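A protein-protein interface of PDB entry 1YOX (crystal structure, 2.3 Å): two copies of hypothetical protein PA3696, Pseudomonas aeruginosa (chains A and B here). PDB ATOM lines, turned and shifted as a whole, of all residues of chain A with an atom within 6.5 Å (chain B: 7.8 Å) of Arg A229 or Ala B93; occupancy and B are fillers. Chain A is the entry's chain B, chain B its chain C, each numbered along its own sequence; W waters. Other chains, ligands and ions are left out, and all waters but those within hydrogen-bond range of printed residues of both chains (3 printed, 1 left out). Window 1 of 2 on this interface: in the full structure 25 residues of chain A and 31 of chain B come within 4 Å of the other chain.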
ATOM      1  N   ASP A 178     -13.695  24.142 -14.449  1.00  0.00           N
ATOM      2  CA  ASP A 178     -13.923  22.727 -14.650  1.00  0.00           C
ATOM      3  C   ASP A 178     -13.685  22.026 -13.311  1.00  0.00           C
ATOM      4  O   ASP A 178     -12.655  22.214 -12.664  1.00  0.00           O
ATOM      5  CB  ASP A 178     -12.965  22.207 -15.708  1.00  0.00           C
ATOM      6  CG  ASP A 178     -13.284  20.777 -16.140  1.00  0.00           C
ATOM      7  OD1 ASP A 178     -12.826  19.860 -15.472  1.00  0.00           O
ATOM      8  OD2 ASP A 178     -13.953  20.570 -17.179  1.00  0.00           O
ATOM      9  N   GLY A 180     -12.913  19.121 -12.023  1.00  0.00           N
ATOM     10  CA  GLY A 180     -11.708  18.338 -11.760  1.00  0.00           C
ATOM     11  C   GLY A 180     -10.436  19.188 -11.700  1.00  0.00           C
ATOM     12  O   GLY A 180      -9.404  18.738 -11.213  1.00  0.00           O
ATOM     13  N   CYS A 181     -10.514  20.412 -12.208  1.00  0.00           N
ATOM     14  CA  CYS A 181      -9.357  21.284 -12.274  1.00  0.00           C
ATOM     15  C   CYS A 181      -9.069  21.912 -10.937  1.00  0.00           C
ATOM     16  O   CYS A 181      -8.031  22.546 -10.788  1.00  0.00           O
ATOM     17  CB  CYS A 181      -9.544  22.383 -13.331  1.00  0.00           C
ATOM     18  SG  CYS A 181      -9.392  21.711 -14.988  1.00  0.00           S
ATOM     19  N   SER A 224      -4.119  21.972 -14.651  1.00  0.00           N
ATOM     20  CA  SER A 224      -4.569  21.984 -16.060  1.00  0.00           C
ATOM     21  C   SER A 224      -4.964  20.612 -16.610  1.00  0.00           C
ATOM     22  O   SER A 224      -5.673  20.542 -17.612  1.00  0.00           O
ATOM     23  CB  SER A 224      -3.484  22.531 -16.974  1.00  0.00           C
ATOM     24  OG  SER A 224      -2.326  21.760 -16.773  1.00  0.00           O
ATOM     25  N   LEU A 225      -4.483  19.540 -15.974  1.00  0.00           N
ATOM     26  CA  LEU A 225      -4.776  18.162 -16.434  1.00  0.00           C
ATOM     27  C   LEU A 225      -5.214  17.255 -15.284  1.00  0.00           C
ATOM     28  O   LEU A 225      -4.454  16.434 -14.787  1.00  0.00           O
ATOM     29  CB  LEU A 225      -3.610  17.550 -17.215  1.00  0.00           C
ATOM     30  CG  LEU A 225      -3.824  16.169 -17.864  1.00  0.00           C
ATOM     31  CD1 LEU A 225      -5.164  16.048 -18.606  1.00  0.00           C
ATOM     32  CD2 LEU A 225      -2.660  15.806 -18.779  1.00  0.00           C
ATOM     33  N   PRO A 226      -6.472  17.396 -14.882  1.00  0.00           N
ATOM     34  CA  PRO A 226      -6.963  16.549 -13.832  1.00  0.00           C
ATOM     35  C   PRO A 226      -6.958  15.083 -14.269  1.00  0.00           C
ATOM     36  O   PRO A 226      -7.217  14.789 -15.453  1.00  0.00           O
ATOM     37  CB  PRO A 226      -8.404  17.040 -13.608  1.00  0.00           C
ATOM     38  CG  PRO A 226      -8.669  18.097 -14.589  1.00  0.00           C
ATOM     39  CD  PRO A 226      -7.484  18.327 -15.430  1.00  0.00           C
ATOM     40  N   PHE A 227      -6.645  14.185 -13.330  1.00  0.00           N
ATOM     41  CA  PHE A 227      -6.753  12.723 -13.539  1.00  0.00           C
ATOM     42  C   PHE A 227      -8.091  12.287 -14.126  1.00  0.00           C
ATOM     43  O   PHE A 227      -8.157  11.424 -15.000  1.00  0.00           O
ATOM     44  CB  PHE A 227      -6.578  12.020 -12.183  1.00  0.00           C
ATOM     45  CG  PHE A 227      -6.553  10.536 -12.261  1.00  0.00           C
ATOM     46  CD1 PHE A 227      -5.467   9.877 -12.843  1.00  0.00           C
ATOM     47  CD2 PHE A 227      -7.591   9.782 -11.728  1.00  0.00           C
ATOM     48  CE1 PHE A 227      -5.410   8.480 -12.903  1.00  0.00           C
ATOM     49  CE2 PHE A 227      -7.553   8.372 -11.795  1.00  0.00           C
ATOM     50  CZ  PHE A 227      -6.456   7.733 -12.373  1.00  0.00           C
ATOM     51  N   SER A 228      -9.163  12.887 -13.623  1.00  0.00           N
ATOM     52  CA  SER A 228     -10.499  12.561 -14.038  1.00  0.00           C
ATOM     53  C   SER A 228     -10.742  12.946 -15.501  1.00  0.00           C
ATOM     54  O   SER A 228     -11.518  12.288 -16.191  1.00  0.00           O
ATOM     55  CB  SER A 228     -11.517  13.255 -13.122  1.00  0.00           C
ATOM     56  OG  SER A 228     -11.528  14.650 -13.379  1.00  0.00           O
ATOM     57  N   ARG A 229     -10.106  14.012 -15.977  1.00  0.00           N
ATOM     58  CA  ARG A 229     -10.229  14.363 -17.385  1.00  0.00           C
ATOM     59  C   ARG A 229      -9.471  13.361 -18.268  1.00  0.00           C
ATOM     60  O   ARG A 229     -10.000  12.853 -19.238  1.00  0.00           O
ATOM     61  CB  ARG A 229      -9.727  15.765 -17.647  1.00  0.00           C
ATOM     62  CG  ARG A 229      -9.948  16.219 -19.058  1.00  0.00           C
ATOM     63  CD  ARG A 229      -9.300  17.564 -19.266  1.00  0.00           C
ATOM     64  NE  ARG A 229     -10.122  18.633 -18.699  1.00  0.00           N
ATOM     65  CZ  ARG A 229      -9.924  19.924 -18.935  1.00  0.00           C
ATOM     66  NH1 ARG A 229      -8.945  20.315 -19.729  1.00  0.00           N
ATOM     67  NH2 ARG A 229     -10.721  20.821 -18.387  1.00  0.00           N
ATOM     68  N   LEU A 230      -8.242  13.091 -17.879  1.00  0.00           N
ATOM     69  CA  LEU A 230      -7.368  12.101 -18.479  1.00  0.00           C
ATOM     70  C   LEU A 230      -8.057  10.713 -18.504  1.00  0.00           C
ATOM     71  O   LEU A 230      -8.181  10.105 -19.558  1.00  0.00           O
ATOM     72  CB  LEU A 230      -6.088  12.027 -17.626  1.00  0.00           C
ATOM     73  CG  LEU A 230      -4.690  11.645 -18.148  1.00  0.00           C
ATOM     74  CD1 LEU A 230      -3.783  11.177 -17.020  1.00  0.00           C
ATOM     75  CD2 LEU A 230      -4.711  10.654 -19.279  1.00  0.00           C
ATOM     76  N   ALA A 231      -8.478  10.229 -17.336  1.00  0.00           N
ATOM     77  CA  ALA A 231      -9.196   8.927 -17.260  1.00  0.00           C
ATOM     78  C   ALA A 231     -10.467   8.930 -18.138  1.00  0.00           C
ATOM     79  O   ALA A 231     -10.592   8.103 -19.066  1.00  0.00           O
ATOM     80  CB  ALA A 231      -9.501   8.542 -15.801  1.00  0.00           C
ATOM     81  N   GLY A 232     -11.363   9.885 -17.897  1.00  0.00           N
ATOM     82  CA  GLY A 232     -12.558  10.057 -18.735  1.00  0.00           C
ATOM     83  C   GLY A 232     -12.371  10.165 -20.245  1.00  0.00           C
ATOM     84  O   GLY A 232     -13.168   9.619 -21.023  1.00  0.00           O
ATOM     85  N   ARG A 233     -11.339  10.884 -20.684  1.00  0.00           N
ATOM     86  CA  ARG A 233     -11.118  11.046 -22.109  1.00  0.00           C
ATOM     87  C   ARG A 233     -10.604   9.747 -22.747  1.00  0.00           C
ATOM     88  O   ARG A 233     -11.023   9.385 -23.835  1.00  0.00           O
ATOM     89  CB  ARG A 233     -10.159  12.213 -22.390  1.00  0.00           C
ATOM     90  CG  ARG A 233      -9.829  12.376 -23.880  1.00  0.00           C
ATOM     91  CD  ARG A 233     -10.963  13.065 -24.656  1.00  0.00           C
ATOM     92  NE  ARG A 233     -11.253  12.425 -25.955  1.00  0.00           N
ATOM     93  CZ  ARG A 233     -10.465  12.485 -27.036  1.00  0.00           C
ATOM     94  NH1 ARG A 233      -9.292  13.160 -26.995  1.00  0.00           N
ATOM     95  NH2 ARG A 233     -10.844  11.870 -28.159  1.00  0.00           N
ATOM     96  N   ILE A 234      -9.675   9.078 -22.065  1.00  0.00           N
ATOM     97  CA  ILE A 234      -9.171   7.760 -22.469  1.00  0.00           C
ATOM     98  C   ILE A 234     -10.313   6.746 -22.570  1.00  0.00           C
ATOM     99  O   ILE A 234     -10.522   6.137 -23.626  1.00  0.00           O
ATOM    100  CB  ILE A 234      -8.102   7.263 -21.462  1.00  0.00           C
ATOM    101  CG1 ILE A 234      -6.780   7.957 -21.730  1.00  0.00           C
ATOM    102  CG2 ILE A 234      -7.938   5.708 -21.475  1.00  0.00           C
ATOM    103  CD1 ILE A 234      -5.730   7.592 -20.716  1.00  0.00           C
ATOM    104  N   MET B  17       4.251  20.598 -19.539  1.00  0.00           N
ATOM    105  CA  MET B  17       2.823  20.417 -19.709  1.00  0.00           C
ATOM    106  C   MET B  17       2.152  21.760 -19.644  1.00  0.00           C
ATOM    107  O   MET B  17       2.332  22.530 -18.690  1.00  0.00           O
ATOM    108  CB  MET B  17       2.254  19.457 -18.683  1.00  0.00           C
ATOM    109  CG  MET B  17       2.578  18.018 -18.968  1.00  0.00           C
ATOM    110  SD  MET B  17       2.247  16.819 -17.441  1.00  0.00           S
ATOM    111  CE  MET B  17       3.600  17.393 -16.184  1.00  0.00           C
ATOM    112  N   GLN B  18       1.363  22.049 -20.667  1.00  0.00           N
ATOM    113  CA  GLN B  18       0.969  23.431 -20.914  1.00  0.00           C
ATOM    114  C   GLN B  18      -0.530  23.679 -21.052  1.00  0.00           C
ATOM    115  O   GLN B  18      -1.308  22.808 -21.520  1.00  0.00           O
ATOM    116  CB  GLN B  18       1.762  23.992 -22.116  1.00  0.00           C
ATOM    117  CG  GLN B  18       3.264  24.048 -21.815  1.00  0.00           C
ATOM    118  CD  GLN B  18       4.126  24.666 -22.914  1.00  0.00           C
ATOM    119  OE1 GLN B  18       3.755  24.717 -24.099  1.00  0.00           O
ATOM    120  NE2 GLN B  18       5.305  25.122 -22.522  1.00  0.00           N
ATOM    121  N   THR B  19      -0.907  24.887 -20.648  1.00  0.00           N
ATOM    122  CA  THR B  19      -2.238  25.417 -20.847  1.00  0.00           C
ATOM    123  C   THR B  19      -2.210  26.868 -21.410  1.00  0.00           C
ATOM    124  O   THR B  19      -1.295  27.628 -21.153  1.00  0.00           O
ATOM    125  CB  THR B  19      -3.021  25.356 -19.546  1.00  0.00           C
ATOM    126  OG1 THR B  19      -4.222  26.124 -19.661  1.00  0.00           O
ATOM    127  CG2 THR B  19      -2.227  25.892 -18.431  1.00  0.00           C
ATOM    128  N   VAL B  20      -3.220  27.230 -22.182  1.00  0.00           N
ATOM    129  CA  VAL B  20      -3.277  28.524 -22.804  1.00  0.00           C
ATOM    130  C   VAL B  20      -4.349  29.400 -22.178  1.00  0.00           C
ATOM    131  O   VAL B  20      -5.533  29.092 -22.206  1.00  0.00           O
ATOM    132  CB  VAL B  20      -3.411  28.444 -24.366  1.00  0.00           C
ATOM    133  CG1 VAL B  20      -4.752  27.869 -24.774  1.00  0.00           C
ATOM    134  CG2 VAL B  20      -3.213  29.837 -24.971  1.00  0.00           C
ATOM    135  N   GLU B  21      -3.909  30.501 -21.596  1.00  0.00           N
ATOM    136  CA  GLU B  21      -4.828  31.446 -21.006  1.00  0.00           C
ATOM    137  C   GLU B  21      -5.003  32.567 -22.013  1.00  0.00           C
ATOM    138  O   GLU B  21      -4.067  33.311 -22.305  1.00  0.00           O
ATOM    139  CB  GLU B  21      -4.327  31.970 -19.659  1.00  0.00           C
ATOM    140  CG  GLU B  21      -5.392  32.782 -18.920  1.00  0.00           C
ATOM    141  CD  GLU B  21      -4.814  33.736 -17.897  1.00  0.00           C
ATOM    142  OE1 GLU B  21      -4.789  33.375 -16.704  1.00  0.00           O
ATOM    143  OE2 GLU B  21      -4.356  34.834 -18.286  1.00  0.00           O
ATOM    144  N   GLU B  33     -13.242  23.426 -28.216  1.00  0.00           N
ATOM    145  CA  GLU B  33     -14.130  22.367 -27.720  1.00  0.00           C
ATOM    146  C   GLU B  33     -14.258  22.586 -26.195  1.00  0.00           C
ATOM    147  O   GLU B  33     -13.269  22.893 -25.509  1.00  0.00           O
ATOM    148  CB  GLU B  33     -13.648  20.955 -28.147  1.00  0.00           C
ATOM    149  CG  GLU B  33     -14.575  19.822 -27.777  1.00  0.00           C
ATOM    150  CD  GLU B  33     -14.534  19.543 -26.285  1.00  0.00           C
ATOM    151  OE1 GLU B  33     -13.413  19.343 -25.735  1.00  0.00           O
ATOM    152  OE2 GLU B  33     -15.617  19.543 -25.658  1.00  0.00           O
ATOM    153  N   ALA B  34     -15.484  22.518 -25.680  1.00  0.00           N
ATOM    154  CA  ALA B  34     -15.740  22.972 -24.286  1.00  0.00           C
ATOM    155  C   ALA B  34     -15.142  22.111 -23.177  1.00  0.00           C
ATOM    156  O   ALA B  34     -15.037  22.579 -22.028  1.00  0.00           O
ATOM    157  CB  ALA B  34     -17.252  23.200 -24.033  1.00  0.00           C
ATOM    158  N   GLY B  35     -14.810  20.853 -23.506  1.00  0.00           N
ATOM    159  CA  GLY B  35     -14.118  19.941 -22.585  1.00  0.00           C
ATOM    160  C   GLY B  35     -12.659  20.315 -22.332  1.00  0.00           C
ATOM    161  O   GLY B  35     -12.049  19.812 -21.406  1.00  0.00           O
ATOM    162  N   ALA B  36     -12.109  21.216 -23.147  1.00  0.00           N
ATOM    163  CA  ALA B  36     -10.767  21.768 -22.926  1.00  0.00           C
ATOM    164  C   ALA B  36     -10.653  22.953 -21.931  1.00  0.00           C
ATOM    165  O   ALA B  36      -9.560  23.234 -21.434  1.00  0.00           O
ATOM    166  CB  ALA B  36     -10.111  22.106 -24.232  1.00  0.00           C
ATOM    167  N   MET B  37     -11.756  23.624 -21.616  1.00  0.00           N
ATOM    168  CA  MET B  37     -11.690  24.764 -20.708  1.00  0.00           C
ATOM    169  C   MET B  37     -11.361  24.365 -19.260  1.00  0.00           C
ATOM    170  O   MET B  37     -11.976  23.438 -18.700  1.00  0.00           O
ATOM    171  CB  MET B  37     -12.985  25.583 -20.761  1.00  0.00           C
ATOM    172  CG  MET B  37     -13.966  25.257 -19.653  1.00  0.00           C
ATOM    173  SD  MET B  37     -13.728  26.388 -18.055  1.00  0.00           S
ATOM    174  CE  MET B  37     -13.736  27.912 -19.152  1.00  0.00           C
ATOM    175  N   ASN B  38     -10.407  25.074 -18.666  1.00  0.00           N
ATOM    176  CA  ASN B  38     -10.035  24.887 -17.253  1.00  0.00           C
ATOM    177  C   ASN B  38     -10.709  25.889 -16.321  1.00  0.00           C
ATOM    178  O   ASN B  38     -11.108  25.524 -15.201  1.00  0.00           O
ATOM    179  CB  ASN B  38      -8.548  25.082 -17.033  1.00  0.00           C
ATOM    180  CG  ASN B  38      -7.681  24.118 -17.810  1.00  0.00           C
ATOM    181  OD1 ASN B  38      -6.583  24.494 -18.213  1.00  0.00           O
ATOM    182  ND2 ASN B  38      -8.124  22.877 -17.985  1.00  0.00           N
ATOM    183  N   TYR B  39     -10.755  27.158 -16.741  1.00  0.00           N
ATOM    184  CA  TYR B  39     -11.334  28.222 -15.943  1.00  0.00           C
ATOM    185  C   TYR B  39     -11.689  29.446 -16.767  1.00  0.00           C
ATOM    186  O   TYR B  39     -11.146  29.682 -17.840  1.00  0.00           O
ATOM    187  CB  TYR B  39     -10.444  28.615 -14.735  1.00  0.00           C
ATOM    188  CG  TYR B  39      -9.125  29.276 -15.106  1.00  0.00           C
ATOM    189  CD1 TYR B  39      -7.947  28.539 -15.098  1.00  0.00           C
ATOM    190  CD2 TYR B  39      -9.057  30.629 -15.473  1.00  0.00           C
ATOM    191  CE1 TYR B  39      -6.741  29.100 -15.443  1.00  0.00           C
ATOM    192  CE2 TYR B  39      -7.820  31.208 -15.839  1.00  0.00           C
ATOM    193  CZ  TYR B  39      -6.669  30.427 -15.810  1.00  0.00           C
ATOM    194  OH  TYR B  39      -5.421  30.927 -16.148  1.00  0.00           O
ATOM    195  N   ALA B  91      -8.947  29.927 -19.795  1.00  0.00           N
ATOM    196  CA  ALA B  91      -7.833  29.023 -20.080  1.00  0.00           C
ATOM    197  C   ALA B  91      -8.281  27.644 -20.655  1.00  0.00           C
ATOM    198  O   ALA B  91      -9.374  27.140 -20.326  1.00  0.00           O
ATOM    199  CB  ALA B  91      -6.942  28.845 -18.838  1.00  0.00           C
ATOM    200  N   PHE B  92      -7.426  27.068 -21.509  1.00  0.00           N
ATOM    201  CA  PHE B  92      -7.695  25.809 -22.209  1.00  0.00           C
ATOM    202  C   PHE B  92      -6.478  24.919 -22.122  1.00  0.00           C
ATOM    203  O   PHE B  92      -5.364  25.429 -22.128  1.00  0.00           O
ATOM    204  CB  PHE B  92      -8.037  26.047 -23.693  1.00  0.00           C
ATOM    205  CG  PHE B  92      -9.205  26.961 -23.896  1.00  0.00           C
ATOM    206  CD1 PHE B  92      -9.000  28.295 -24.262  1.00  0.00           C
ATOM    207  CD2 PHE B  92     -10.501  26.502 -23.689  1.00  0.00           C
ATOM    208  CE1 PHE B  92     -10.048  29.147 -24.434  1.00  0.00           C
ATOM    209  CE2 PHE B  92     -11.588  27.341 -23.849  1.00  0.00           C
ATOM    210  CZ  PHE B  92     -11.374  28.675 -24.238  1.00  0.00           C
ATOM    211  N   ALA B  93      -6.707  23.603 -21.997  1.00  0.00           N
ATOM    212  CA  ALA B  93      -5.654  22.558 -22.057  1.00  0.00           C
ATOM    213  C   ALA B  93      -6.217  21.268 -22.677  1.00  0.00           C
ATOM    214  O   ALA B  93      -7.416  20.945 -22.523  1.00  0.00           O
ATOM    215  CB  ALA B  93      -5.095  22.267 -20.702  1.00  0.00           C
ATOM    216  N   ALA B  94      -5.357  20.543 -23.394  1.00  0.00           N
ATOM    217  CA  ALA B  94      -5.734  19.238 -23.957  1.00  0.00           C
ATOM    218  C   ALA B  94      -5.850  18.184 -22.828  1.00  0.00           C
ATOM    219  O   ALA B  94      -5.297  18.374 -21.744  1.00  0.00           O
ATOM    220  CB  ALA B  94      -4.732  18.812 -25.008  1.00  0.00           C
ATOM    221  N   PRO B  95      -6.579  17.071 -23.080  1.00  0.00           N
ATOM    222  CA  PRO B  95      -6.741  16.053 -22.035  1.00  0.00           C
ATOM    223  C   PRO B  95      -5.650  14.997 -21.972  1.00  0.00           C
ATOM    224  O   PRO B  95      -5.901  13.879 -21.506  1.00  0.00           O
ATOM    225  CB  PRO B  95      -8.101  15.440 -22.359  1.00  0.00           C
ATOM    226  CG  PRO B  95      -8.298  15.669 -23.867  1.00  0.00           C
ATOM    227  CD  PRO B  95      -7.318  16.726 -24.323  1.00  0.00           C
ATOM    228  N   TYR B  96      -4.444  15.338 -22.419  1.00  0.00           N
ATOM    229  CA  TYR B  96      -3.278  14.447 -22.292  1.00  0.00           C
ATOM    230  C   TYR B  96      -2.030  15.343 -22.239  1.00  0.00           C
ATOM    231  O   TYR B  96      -2.084  16.486 -22.711  1.00  0.00           O
ATOM    232  CB  TYR B  96      -3.220  13.410 -23.434  1.00  0.00           C
ATOM    233  CG  TYR B  96      -3.387  13.981 -24.817  1.00  0.00           C
ATOM    234  CD1 TYR B  96      -2.286  14.303 -25.600  1.00  0.00           C
ATOM    235  CD2 TYR B  96      -4.657  14.200 -25.346  1.00  0.00           C
ATOM    236  CE1 TYR B  96      -2.441  14.850 -26.878  1.00  0.00           C
ATOM    237  CE2 TYR B  96      -4.823  14.745 -26.599  1.00  0.00           C
ATOM    238  CZ  TYR B  96      -3.719  15.078 -27.349  1.00  0.00           C
ATOM    239  OH  TYR B  96      -3.927  15.612 -28.592  1.00  0.00           O
ATOM    240  N   GLY B  98       1.452  17.381 -22.512  1.00  0.00           N
ATOM    241  CA  GLY B  98       2.263  17.894 -23.583  1.00  0.00           C
ATOM    242  C   GLY B  98       2.160  19.393 -23.688  1.00  0.00           C
ATOM    243  O   GLY B  98       1.559  20.040 -22.838  1.00  0.00           O
ATOM    244  N   VAL B 100       1.811  23.350 -25.695  1.00  0.00           N
ATOM    245  CA  VAL B 100       0.906  24.126 -26.507  1.00  0.00           C
ATOM    246  C   VAL B 100       1.786  24.947 -27.449  1.00  0.00           C
ATOM    247  O   VAL B 100       2.869  25.351 -27.072  1.00  0.00           O
ATOM    248  CB  VAL B 100       0.017  25.021 -25.599  1.00  0.00           C
ATOM    249  CG1 VAL B 100      -0.885  25.916 -26.400  1.00  0.00           C
ATOM    250  CG2 VAL B 100      -0.810  24.143 -24.617  1.00  0.00           C
ATOM    251  N   PHE B 119      -6.114  19.944 -32.064  1.00  0.00           N
ATOM    252  CA  PHE B 119      -6.740  21.261 -31.974  1.00  0.00           C
ATOM    253  C   PHE B 119      -7.056  21.655 -30.514  1.00  0.00           C
ATOM    254  O   PHE B 119      -7.710  20.908 -29.793  1.00  0.00           O
ATOM    255  CB  PHE B 119      -7.996  21.360 -32.857  1.00  0.00           C
ATOM    256  CG  PHE B 119      -8.713  22.675 -32.726  1.00  0.00           C
ATOM    257  CD1 PHE B 119      -8.240  23.810 -33.385  1.00  0.00           C
ATOM    258  CD2 PHE B 119      -9.824  22.804 -31.890  1.00  0.00           C
ATOM    259  CE1 PHE B 119      -8.899  25.058 -33.251  1.00  0.00           C
ATOM    260  CE2 PHE B 119     -10.481  24.056 -31.748  1.00  0.00           C
ATOM    261  CZ  PHE B 119     -10.016  25.169 -32.432  1.00  0.00           C
ATOM    262  N   LEU B 120      -6.576  22.812 -30.077  1.00  0.00           N
ATOM    263  CA  LEU B 120      -6.883  23.320 -28.726  1.00  0.00           C
ATOM    264  C   LEU B 120      -7.883  24.493 -28.721  1.00  0.00           C
ATOM    265  O   LEU B 120      -8.973  24.387 -28.143  1.00  0.00           O
ATOM    266  CB  LEU B 120      -5.601  23.687 -27.956  1.00  0.00           C
ATOM    267  CG  LEU B 120      -5.810  24.128 -26.509  1.00  0.00           C
ATOM    268  CD1 LEU B 120      -6.739  23.127 -25.787  1.00  0.00           C
ATOM    269  CD2 LEU B 120      -4.480  24.253 -25.795  1.00  0.00           C
ATOM    270  N   CYS B 121      -7.511  25.615 -29.329  1.00  0.00           N
ATOM    271  CA  CYS B 121      -8.478  26.705 -29.545  1.00  0.00           C
ATOM    272  C   CYS B 121      -8.021  27.663 -30.626  1.00  0.00           C
ATOM    273  O   CYS B 121      -6.871  27.604 -31.093  1.00  0.00           O
ATOM    274  CB  CYS B 121      -8.761  27.489 -28.252  1.00  0.00           C
ATOM    275  SG  CYS B 121      -7.289  28.137 -27.558  1.00  0.00           S
ATOM    276  N   HIS B 160      -1.982  21.461 -29.775  1.00  0.00           N
ATOM    277  CA  HIS B 160      -1.300  20.791 -28.686  1.00  0.00           C
ATOM    278  C   HIS B 160      -0.512  19.555 -29.173  1.00  0.00           C
ATOM    279  O   HIS B 160      -1.038  18.759 -29.944  1.00  0.00           O
ATOM    280  CB  HIS B 160      -2.361  20.407 -27.646  1.00  0.00           C
ATOM    281  CG  HIS B 160      -1.867  19.487 -26.576  1.00  0.00           C
ATOM    282  ND1 HIS B 160      -1.472  19.940 -25.335  1.00  0.00           N
ATOM    283  CD2 HIS B 160      -1.732  18.139 -26.546  1.00  0.00           C
ATOM    284  CE1 HIS B 160      -1.122  18.910 -24.582  1.00  0.00           C
ATOM    285  NE2 HIS B 160      -1.265  17.807 -25.294  1.00  0.00           N
ATOM    286  N   PHE B 227      -2.089  11.010 -28.161  1.00  0.00           N
ATOM    287  CA  PHE B 227      -3.144  10.503 -27.319  1.00  0.00           C
ATOM    288  C   PHE B 227      -3.534   9.071 -27.718  1.00  0.00           C
ATOM    289  O   PHE B 227      -3.928   8.245 -26.870  1.00  0.00           O
ATOM    290  CB  PHE B 227      -4.350  11.440 -27.437  1.00  0.00           C
ATOM    291  CG  PHE B 227      -5.590  10.927 -26.768  1.00  0.00           C
ATOM    292  CD1 PHE B 227      -5.663  10.825 -25.387  1.00  0.00           C
ATOM    293  CD2 PHE B 227      -6.693  10.570 -27.522  1.00  0.00           C
ATOM    294  CE1 PHE B 227      -6.796  10.376 -24.776  1.00  0.00           C
ATOM    295  CE2 PHE B 227      -7.837  10.122 -26.910  1.00  0.00           C
ATOM    296  CZ  PHE B 227      -7.886  10.004 -25.544  1.00  0.00           C
HETATM  297  O   HOH W   1      -6.734  19.050 -19.475  1.00  0.00           O
HETATM  298  O   HOH W   2      -9.640  18.659 -22.615  1.00  0.00           O
HETATM  299  O   HOH W   3     -13.503  18.888 -19.223  1.00  0.00           O
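Water W1 lies within hydrogen-bond range of NH1 of Arg A229 (2.6 Å), O of Ser A224 (2.6 Å) and O of Ala B94 (2.8 Å). Water W3 lies within hydrogen-bond range of OD2 of Asp A178, O of Gly B35 and NE of Arg A229. Water W2 lies within hydrogen-bond range of the backbone carbonyl oxygen (O) of Gly B35 (2.9 Å), the backbone carbonyl oxygen (O) of Ala B93 (3.2 Å) and the guanidinium group (NH1) of Arg A229 (3.4 Å).
Of the 14 printed residues of chain A, 8 touch a printed residue of chain B. Hydrophobic or aromatic side chains of chain A within 4 Å of the printed part of chain B: Leu A225 and Ile A234. Printed residues of chain B that touch a printed residue of chain A: Thr B19, Gly B35, Ala B36, Met B37, Asn B38, Ala B93, Ala B94, Pro B95, Tyr B96 and Phe B227. Among the printed residues, 19 pairs touch across the chains. Among the printed residues, no Asp or Glu carboxylate lies within 4 Å of a Lys or Arg side-chain nitrogen of the other chain.
Of chain B, only Gly B35 (3.3 Å), Ala B36 (3.4 Å), Met B37 (2.9 Å), Asn B38 (3.2 Å), Ala B93 (3.2 Å) and Pro B95 (3.9 Å) come within 4 Å of Arg A229. Ala B93 touches just these residues of chain A: Ser A224 and Arg A229. Of the printed residues of chain A, Phe B227 touches Arg A233 (3.4 Å) and Ile A234 (3.9 Å). Of the printed residues of chain B, Asp A178 touches Met B37 and Asn B38.
Among the printed residues, merely in contact across the chains: Arg A233 with Phe B227 (3.4 Å), Asp A178 with Met B37 (3.4 Å), Leu A225 with Tyr B96 (3.5 Å), Leu A225 with Pro B95 (3.6 Å), Ser A224 with Ala B93 (3.6 Å), Arg A233 with Pro B95 (3.6 Å), Leu A230 with Pro B95 (3.8 Å), Ser A224 with Thr B19 (3.8 Å), Arg A229 with Pro B95 (3.9 Å), Ile A234 with Phe B227 (3.9 Å) and Leu A225 with Ala B94 (3.9 Å).
Position printed for both chains: 227. Of the 19 pairs that touch across the chains among the printed residues, none has its exchanged pair printed and touching as well.
N of Asn B38 sits at hydrogen-bond distance from O of Ala B91 (2.8 Å). The guanidinium group (NH2) of Arg A229 is in salt-bridge range of the side-chain carboxylate (OD2) of Asp A178 (3.5 Å). O of Tyr B96 sits at hydrogen-bond distance from NE2 of His B160, at 3.0 Å. O of Phe B92 is in hydrogen-bond range of OG1 of Thr B19. The side-chain sulfur (SG) of Cys A181 is in hydrogen-bond range of the guanidinium group (NH2) of Arg A229 (3.8 Å). O of Ala B36 sits at hydrogen-bond distance from N of Ala B93, 2.9 Å away.
O of Met B37 sits at hydrogen-bond distance from NH2 of Arg A229 (2.9 Å). The backbone carbonyl oxygen of Gly B35 sits close to the guanidinium group of Arg A229, at 3.4 Å. O of Ser A224 sits at hydrogen-bond distance from ND2 of Asn B38 (3.4 Å). NH1 of Arg A229 lies within hydrogen-bond range of O of Ala B36, 3.4 Å away. The side-chain sulfur (SG) of Cys A181 lies within hydrogen-bond range of the side-chain amide nitrogen (ND2) of Asn B38 (3.5 Å). NH1 of Arg A229 lies within hydrogen-bond range of O of Ala B93 (3.2 Å). NH1 of Arg A229 sits close to ND2 of Asn B38, at 3.2 Å. N of Asp A178 sits at hydrogen-bond distance from O of Asn B38 (3.0 Å).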
